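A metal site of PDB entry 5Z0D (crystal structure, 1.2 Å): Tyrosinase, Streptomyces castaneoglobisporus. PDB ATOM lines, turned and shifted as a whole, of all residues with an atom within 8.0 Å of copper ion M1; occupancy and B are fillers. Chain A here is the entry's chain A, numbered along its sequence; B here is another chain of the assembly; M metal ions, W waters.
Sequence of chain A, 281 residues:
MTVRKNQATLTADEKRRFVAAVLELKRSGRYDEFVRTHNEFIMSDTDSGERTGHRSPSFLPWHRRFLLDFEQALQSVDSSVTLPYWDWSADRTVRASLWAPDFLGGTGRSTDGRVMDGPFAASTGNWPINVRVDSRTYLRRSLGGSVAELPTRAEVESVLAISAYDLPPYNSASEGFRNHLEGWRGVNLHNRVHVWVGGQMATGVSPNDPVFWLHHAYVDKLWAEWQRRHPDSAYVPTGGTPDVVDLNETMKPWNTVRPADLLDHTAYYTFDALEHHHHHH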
ATOM      1  N   HIS A  38       7.422  28.515   6.992  1.00  0.00           N
ATOM      2  CA  HIS A  38       8.314  28.741   5.867  1.00  0.00           C
ATOM      3  C   HIS A  38       7.685  29.670   4.837  1.00  0.00           C
ATOM      4  O   HIS A  38       8.344  30.640   4.375  1.00  0.00           O
ATOM      5  CB  HIS A  38       8.689  27.400   5.209  1.00  0.00           C
ATOM      6  CG  HIS A  38       9.784  27.636   4.206  1.00  0.00           C
ATOM      7  ND1 HIS A  38       9.597  27.776   2.861  1.00  0.00           N
ATOM      8  CD2 HIS A  38      11.105  27.786   4.434  1.00  0.00           C
ATOM      9  CE1 HIS A  38      10.790  28.004   2.284  1.00  0.00           C
ATOM     10  NE2 HIS A  38      11.760  28.017   3.227  1.00  0.00           N
ATOM     11  N   ILE A  42       8.861  33.241   3.287  1.00  0.00           N
ATOM     12  CA  ILE A  42       9.050  33.436   1.856  1.00  0.00           C
ATOM     13  C   ILE A  42       8.301  34.630   1.371  1.00  0.00           C
ATOM     14  O   ILE A  42       8.806  35.440   0.543  1.00  0.00           O
ATOM     15  CB  ILE A  42       8.628  32.142   1.075  1.00  0.00           C
ATOM     16  CG1 ILE A  42       9.630  31.019   1.255  1.00  0.00           C
ATOM     17  CG2 ILE A  42       8.315  32.418  -0.419  1.00  0.00           C
ATOM     18  CD1 ILE A  42      10.925  31.210   0.477  1.00  0.00           C
ATOM     19  N   GLY A  53      14.706  35.218   6.685  1.00  0.00           N
ATOM     20  CA  GLY A  53      14.957  33.816   6.366  1.00  0.00           C
ATOM     21  C   GLY A  53      15.649  33.623   5.032  1.00  0.00           C
ATOM     22  O   GLY A  53      16.247  32.570   4.817  1.00  0.00           O
ATOM     23  N   HIS A  54      15.514  34.577   4.110  1.00  0.00           N
ATOM     24  CA  HIS A  54      15.920  34.384   2.715  1.00  0.00           C
ATOM     25  C   HIS A  54      16.522  35.707   2.208  1.00  0.00           C
ATOM     26  O   HIS A  54      16.326  36.763   2.833  1.00  0.00           O
ATOM     27  CB  HIS A  54      14.693  34.026   1.797  1.00  0.00           C
ATOM     28  CG  HIS A  54      14.022  32.762   2.326  1.00  0.00           C
ATOM     29  ND1 HIS A  54      13.023  32.823   3.306  1.00  0.00           N
ATOM     30  CD2 HIS A  54      14.264  31.449   2.115  1.00  0.00           C
ATOM     31  CE1 HIS A  54      12.680  31.577   3.615  1.00  0.00           C
ATOM     32  NE2 HIS A  54      13.411  30.703   2.898  1.00  0.00           N
ATOM     33  N   PHE A  59      19.944  34.030   5.778  1.00  0.00           N
ATOM     34  CA  PHE A  59      19.476  32.821   5.106  1.00  0.00           C
ATOM     35  C   PHE A  59      20.124  31.561   5.699  1.00  0.00           C
ATOM     36  O   PHE A  59      19.433  30.570   5.971  1.00  0.00           O
ATOM     37  CB  PHE A  59      19.849  32.939   3.611  1.00  0.00           C
ATOM     38  CG  PHE A  59      19.665  31.683   2.780  1.00  0.00           C
ATOM     39  CD1 PHE A  59      18.402  31.160   2.509  1.00  0.00           C
ATOM     40  CD2 PHE A  59      20.787  31.036   2.248  1.00  0.00           C
ATOM     41  CE1 PHE A  59      18.240  30.060   1.690  1.00  0.00           C
ATOM     42  CE2 PHE A  59      20.632  29.905   1.435  1.00  0.00           C
ATOM     43  CZ  PHE A  59      19.352  29.416   1.184  1.00  0.00           C
ATOM     44  N   HIS A  63      18.037  28.993   8.219  1.00  0.00           N
ATOM     45  CA  HIS A  63      17.713  27.607   7.858  1.00  0.00           C
ATOM     46  C   HIS A  63      18.417  26.613   8.741  1.00  0.00           C
ATOM     47  O   HIS A  63      17.890  25.520   8.962  1.00  0.00           O
ATOM     48  CB  HIS A  63      18.027  27.363   6.354  1.00  0.00           C
ATOM     49  CG  HIS A  63      16.991  27.995   5.473  1.00  0.00           C
ATOM     50  ND1 HIS A  63      17.025  29.337   5.122  1.00  0.00           N
ATOM     51  CD2 HIS A  63      15.865  27.500   4.892  1.00  0.00           C
ATOM     52  CE1 HIS A  63      15.975  29.611   4.352  1.00  0.00           C
ATOM     53  NE2 HIS A  63      15.196  28.518   4.169  1.00  0.00           N
ATOM     54  N   GLU A 182      22.886  30.762  -2.187  1.00  0.00           N
ATOM     55  CA  GLU A 182      21.423  30.831  -2.287  1.00  0.00           C
ATOM     56  C   GLU A 182      20.984  30.747  -3.716  1.00  0.00           C
ATOM     57  O   GLU A 182      20.032  30.017  -4.059  1.00  0.00           O
ATOM     58  CB  GLU A 182      20.991  32.129  -1.552  1.00  0.00           C
ATOM     59  CG  GLU A 182      19.419  32.130  -1.426  1.00  0.00           C
ATOM     60  CD  GLU A 182      18.944  33.310  -0.596  1.00  0.00           C
ATOM     61  OE1 GLU A 182      19.758  34.122  -0.068  1.00  0.00           O
ATOM     62  OE2 GLU A 182      17.671  33.412  -0.520  1.00  0.00           O
ATOM     63  N   HIS A 190      21.421  26.818  -4.721  1.00  0.00           N
ATOM     64  CA  HIS A 190      20.245  26.364  -3.969  1.00  0.00           C
ATOM     65  C   HIS A 190      18.919  26.615  -4.674  1.00  0.00           C
ATOM     66  O   HIS A 190      18.048  25.741  -4.657  1.00  0.00           O
ATOM     67  CB  HIS A 190      20.276  27.034  -2.567  1.00  0.00           C
ATOM     68  CG  HIS A 190      18.927  27.271  -1.962  1.00  0.00           C
ATOM     69  ND1 HIS A 190      18.186  28.394  -2.300  1.00  0.00           N
ATOM     70  CD2 HIS A 190      18.212  26.564  -1.090  1.00  0.00           C
ATOM     71  CE1 HIS A 190      17.017  28.342  -1.600  1.00  0.00           C
ATOM     72  NE2 HIS A 190      16.987  27.224  -0.859  1.00  0.00           N
ATOM     73  N   ASN A 191      18.768  27.752  -5.337  1.00  0.00           N
ATOM     74  CA  ASN A 191      17.483  28.012  -5.999  1.00  0.00           C
ATOM     75  C   ASN A 191      17.267  27.060  -7.154  1.00  0.00           C
ATOM     76  O   ASN A 191      16.157  26.547  -7.336  1.00  0.00           O
ATOM     77  CB  ASN A 191      17.429  29.455  -6.527  1.00  0.00           C
ATOM     78  CG  ASN A 191      17.258  30.492  -5.455  1.00  0.00           C
ATOM     79  OD1 ASN A 191      17.026  30.229  -4.279  1.00  0.00           O
ATOM     80  ND2 ASN A 191      17.339  31.760  -5.887  1.00  0.00           N
ATOM     81  N   VAL A 193      18.203  24.010  -7.462  1.00  0.00           N
ATOM     82  CA  VAL A 193      17.761  22.686  -7.013  1.00  0.00           C
ATOM     83  C   VAL A 193      16.257  22.667  -6.770  1.00  0.00           C
ATOM     84  O   VAL A 193      15.556  21.735  -7.117  1.00  0.00           O
ATOM     85  CB  VAL A 193      18.538  22.285  -5.766  1.00  0.00           C
ATOM     86  CG1 VAL A 193      18.003  20.963  -5.221  1.00  0.00           C
ATOM     87  CG2 VAL A 193      20.039  22.166  -6.077  1.00  0.00           C
ATOM     88  N   HIS A 194      15.728  23.742  -6.127  1.00  0.00           N
ATOM     89  CA  HIS A 194      14.270  23.858  -5.982  1.00  0.00           C
ATOM     90  C   HIS A 194      13.583  23.756  -7.321  1.00  0.00           C
ATOM     91  O   HIS A 194      12.561  23.036  -7.495  1.00  0.00           O
ATOM     92  CB  HIS A 194      13.934  25.178  -5.285  1.00  0.00           C
ATOM     93  CG  HIS A 194      14.071  25.245  -3.823  1.00  0.00           C
ATOM     94  ND1 HIS A 194      13.032  24.781  -3.001  1.00  0.00           N
ATOM     95  CD2 HIS A 194      15.002  25.748  -2.987  1.00  0.00           C
ATOM     96  CE1 HIS A 194      13.398  25.028  -1.759  1.00  0.00           C
ATOM     97  NE2 HIS A 194      14.599  25.599  -1.649  1.00  0.00           N
ATOM     98  N   MET A 201       8.257  21.800  -4.312  1.00  0.00           N
ATOM     99  CA  MET A 201       9.602  22.313  -4.063  1.00  0.00           C
ATOM    100  C   MET A 201       9.886  23.580  -4.847  1.00  0.00           C
ATOM    101  O   MET A 201      10.797  24.321  -4.496  1.00  0.00           O
ATOM    102  CB  MET A 201      10.606  21.217  -4.472  1.00  0.00           C
ATOM    103  CG  MET A 201      11.020  20.394  -3.310  1.00  0.00           C
ATOM    104  SD  MET A 201      11.984  21.222  -2.025  1.00  0.00           S
ATOM    105  CE  MET A 201      13.617  21.251  -2.713  1.00  0.00           C
ATOM    106  N   THR A 203       7.891  26.153  -4.940  1.00  0.00           N
ATOM    107  CA  THR A 203       6.987  27.132  -4.386  1.00  0.00           C
ATOM    108  C   THR A 203       7.411  27.536  -2.968  1.00  0.00           C
ATOM    109  O   THR A 203       8.289  26.914  -2.353  1.00  0.00           O
ATOM    110  CB  THR A 203       5.553  26.603  -4.287  1.00  0.00           C
ATOM    111  OG1 THR A 203       5.458  25.677  -3.161  1.00  0.00           O
ATOM    112  CG2 THR A 203       5.154  25.832  -5.563  1.00  0.00           C
ATOM    113  N   SER A 206       7.523  24.845  -0.223  1.00  0.00           N
ATOM    114  CA  SER A 206       8.488  23.772  -0.558  1.00  0.00           C
ATOM    115  C   SER A 206       8.725  22.761   0.556  1.00  0.00           C
ATOM    116  O   SER A 206       8.983  21.607   0.205  1.00  0.00           O
ATOM    117  CB  SER A 206       9.796  24.408  -1.052  1.00  0.00           C
ATOM    118  OG  SER A 206      10.290  25.388  -0.157  1.00  0.00           O
ATOM    119  N   PRO A 207       8.592  23.072   1.860  1.00  0.00           N
ATOM    120  CA  PRO A 207       8.748  22.002   2.855  1.00  0.00           C
ATOM    121  C   PRO A 207       7.653  20.963   2.775  1.00  0.00           C
ATOM    122  O   PRO A 207       7.769  19.949   3.480  1.00  0.00           O
ATOM    123  CB  PRO A 207       8.752  22.714   4.213  1.00  0.00           C
ATOM    124  CG  PRO A 207       9.231  24.163   3.867  1.00  0.00           C
ATOM    125  CD  PRO A 207       8.571  24.394   2.530  1.00  0.00           C
ATOM    126  N   PHE A 212      12.934  18.696   0.885  1.00  0.00           N
ATOM    127  CA  PHE A 212      13.339  20.028   1.317  1.00  0.00           C
ATOM    128  C   PHE A 212      14.421  19.943   2.363  1.00  0.00           C
ATOM    129  O   PHE A 212      15.389  20.696   2.356  1.00  0.00           O
ATOM    130  CB  PHE A 212      12.063  20.738   1.849  1.00  0.00           C
ATOM    131  CG  PHE A 212      12.371  22.054   2.543  1.00  0.00           C
ATOM    132  CD1 PHE A 212      12.674  22.200   3.865  1.00  0.00           C
ATOM    133  CD2 PHE A 212      12.353  23.231   1.741  1.00  0.00           C
ATOM    134  CE1 PHE A 212      13.041  23.426   4.447  1.00  0.00           C
ATOM    135  CE2 PHE A 212      12.666  24.459   2.304  1.00  0.00           C
ATOM    136  CZ  PHE A 212      12.975  24.562   3.641  1.00  0.00           C
ATOM    137  N   HIS A 215      17.781  18.743   1.019  1.00  0.00           N
ATOM    138  CA  HIS A 215      18.426  19.823   0.246  1.00  0.00           C
ATOM    139  C   HIS A 215      19.035  20.829   1.208  1.00  0.00           C
ATOM    140  O   HIS A 215      20.249  21.176   1.099  1.00  0.00           O
ATOM    141  CB  HIS A 215      17.349  20.465  -0.627  1.00  0.00           C
ATOM    142  CG  HIS A 215      17.761  21.706  -1.364  1.00  0.00           C
ATOM    143  ND1 HIS A 215      19.060  21.814  -1.845  1.00  0.00           N
ATOM    144  CD2 HIS A 215      17.070  22.816  -1.736  1.00  0.00           C
ATOM    145  CE1 HIS A 215      19.115  22.964  -2.491  1.00  0.00           C
ATOM    146  NE2 HIS A 215      17.959  23.601  -2.459  1.00  0.00           N
ATOM    147  N   HIS A 216      18.237  21.319   2.148  1.00  0.00           N
ATOM    148  CA  HIS A 216      18.806  22.306   3.075  1.00  0.00           C
ATOM    149  C   HIS A 216      19.842  21.740   3.986  1.00  0.00           C
ATOM    150  O   HIS A 216      20.739  22.504   4.390  1.00  0.00           O
ATOM    151  CB  HIS A 216      17.670  23.028   3.864  1.00  0.00           C
ATOM    152  CG  HIS A 216      17.211  24.187   3.033  1.00  0.00           C
ATOM    153  ND1 HIS A 216      17.883  25.411   3.088  1.00  0.00           N
ATOM    154  CD2 HIS A 216      16.249  24.327   2.120  1.00  0.00           C
ATOM    155  CE1 HIS A 216      17.304  26.252   2.175  1.00  0.00           C
ATOM    156  NE2 HIS A 216      16.296  25.601   1.570  1.00  0.00           N
ATOM    157  N   VAL A 219      22.864  22.251   1.767  1.00  0.00           N
ATOM    158  CA  VAL A 219      23.228  23.702   1.765  1.00  0.00           C
ATOM    159  C   VAL A 219      23.911  24.066   3.066  1.00  0.00           C
ATOM    160  O   VAL A 219      24.900  24.815   3.104  1.00  0.00           O
ATOM    161  CB  VAL A 219      21.957  24.535   1.540  1.00  0.00           C
ATOM    162  CG1 VAL A 219      22.208  26.020   1.721  1.00  0.00           C
ATOM    163  CG2 VAL A 219      21.333  24.261   0.144  1.00  0.00           C
ATOM    164  N   HIS B  97       8.701  30.484  -7.019  1.00  0.00           N
ATOM    165  CA  HIS B  97       9.395  31.489  -6.201  1.00  0.00           C
ATOM    166  C   HIS B  97      10.887  31.510  -6.515  1.00  0.00           C
ATOM    167  O   HIS B  97      11.527  32.535  -6.185  1.00  0.00           O
ATOM    168  CB  HIS B  97       9.133  31.074  -4.732  1.00  0.00           C
ATOM    169  CG  HIS B  97       9.922  31.985  -3.870  1.00  0.00           C
ATOM    170  ND1 HIS B  97       9.491  33.212  -3.557  1.00  0.00           N
ATOM    171  CD2 HIS B  97      11.128  31.946  -3.269  1.00  0.00           C
ATOM    172  CE1 HIS B  97      10.259  33.933  -2.824  1.00  0.00           C
ATOM    173  NE2 HIS B  97      11.301  33.146  -2.661  1.00  0.00           N
ATOM    174  N   TYR B  98      11.432  30.468  -7.074  1.00  0.00           N
ATOM    175  CA  TYR B  98      12.904  30.327  -7.143  1.00  0.00           C
ATOM    176  C   TYR B  98      13.375  30.558  -8.550  1.00  0.00           C
ATOM    177  O   TYR B  98      14.550  30.310  -8.793  1.00  0.00           O
ATOM    178  CB  TYR B  98      13.357  28.936  -6.618  1.00  0.00           C
ATOM    179  CG  TYR B  98      12.905  28.646  -5.192  1.00  0.00           C
ATOM    180  CD1 TYR B  98      11.733  27.970  -4.910  1.00  0.00           C
ATOM    181  CD2 TYR B  98      13.646  29.097  -4.099  1.00  0.00           C
ATOM    182  CE1 TYR B  98      11.329  27.725  -3.607  1.00  0.00           C
ATOM    183  CE2 TYR B  98      13.233  28.818  -2.795  1.00  0.00           C
ATOM    184  CZ  TYR B  98      12.099  28.145  -2.516  1.00  0.00           C
ATOM    185  OH  TYR B  98      11.673  27.868  -1.248  1.00  0.00           O
HETATM  186 CU    CU M   1      15.382  26.339  -0.011  1.00  0.00          CU
HETATM  187 CU    CU M   2      13.581  28.633   3.132  1.00  0.00          CU
HETATM  188  O   HOH W   1      14.081  28.252   0.654  1.00  0.00           O
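A ring nitrogen (ND1) of His 190 sits at hydrogen-bond distance from the side-chain amide oxygen of Asn 191 (2.9 Å).
A ring nitrogen (ND1) of His 190 lies within hydrogen-bond range of the backbone carbonyl oxygen (O) of Glu 182 (3.0 Å).
The backbone carbonyl oxygen (O) of His 190 lies within hydrogen-bond range of a ring nitrogen (NE2) of His 215.
O of Met 201 lies within hydrogen-bond range of ND1 of His 194.
Copper ion M1 is bound by a ring nitrogen (NE2) of His 194 (2.0 Å), a ring nitrogen (NE2) of His 216 (2.0 Å), a ring nitrogen (NE2) of His 190 (2.0 Å) and water W1 (2.4 Å).
Of the 21 residues printed, 3 come within 4 Å of copper ion M1.
The nearest printed residue that does not touch copper ion M1 is Phe 212 (4.03 Å).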
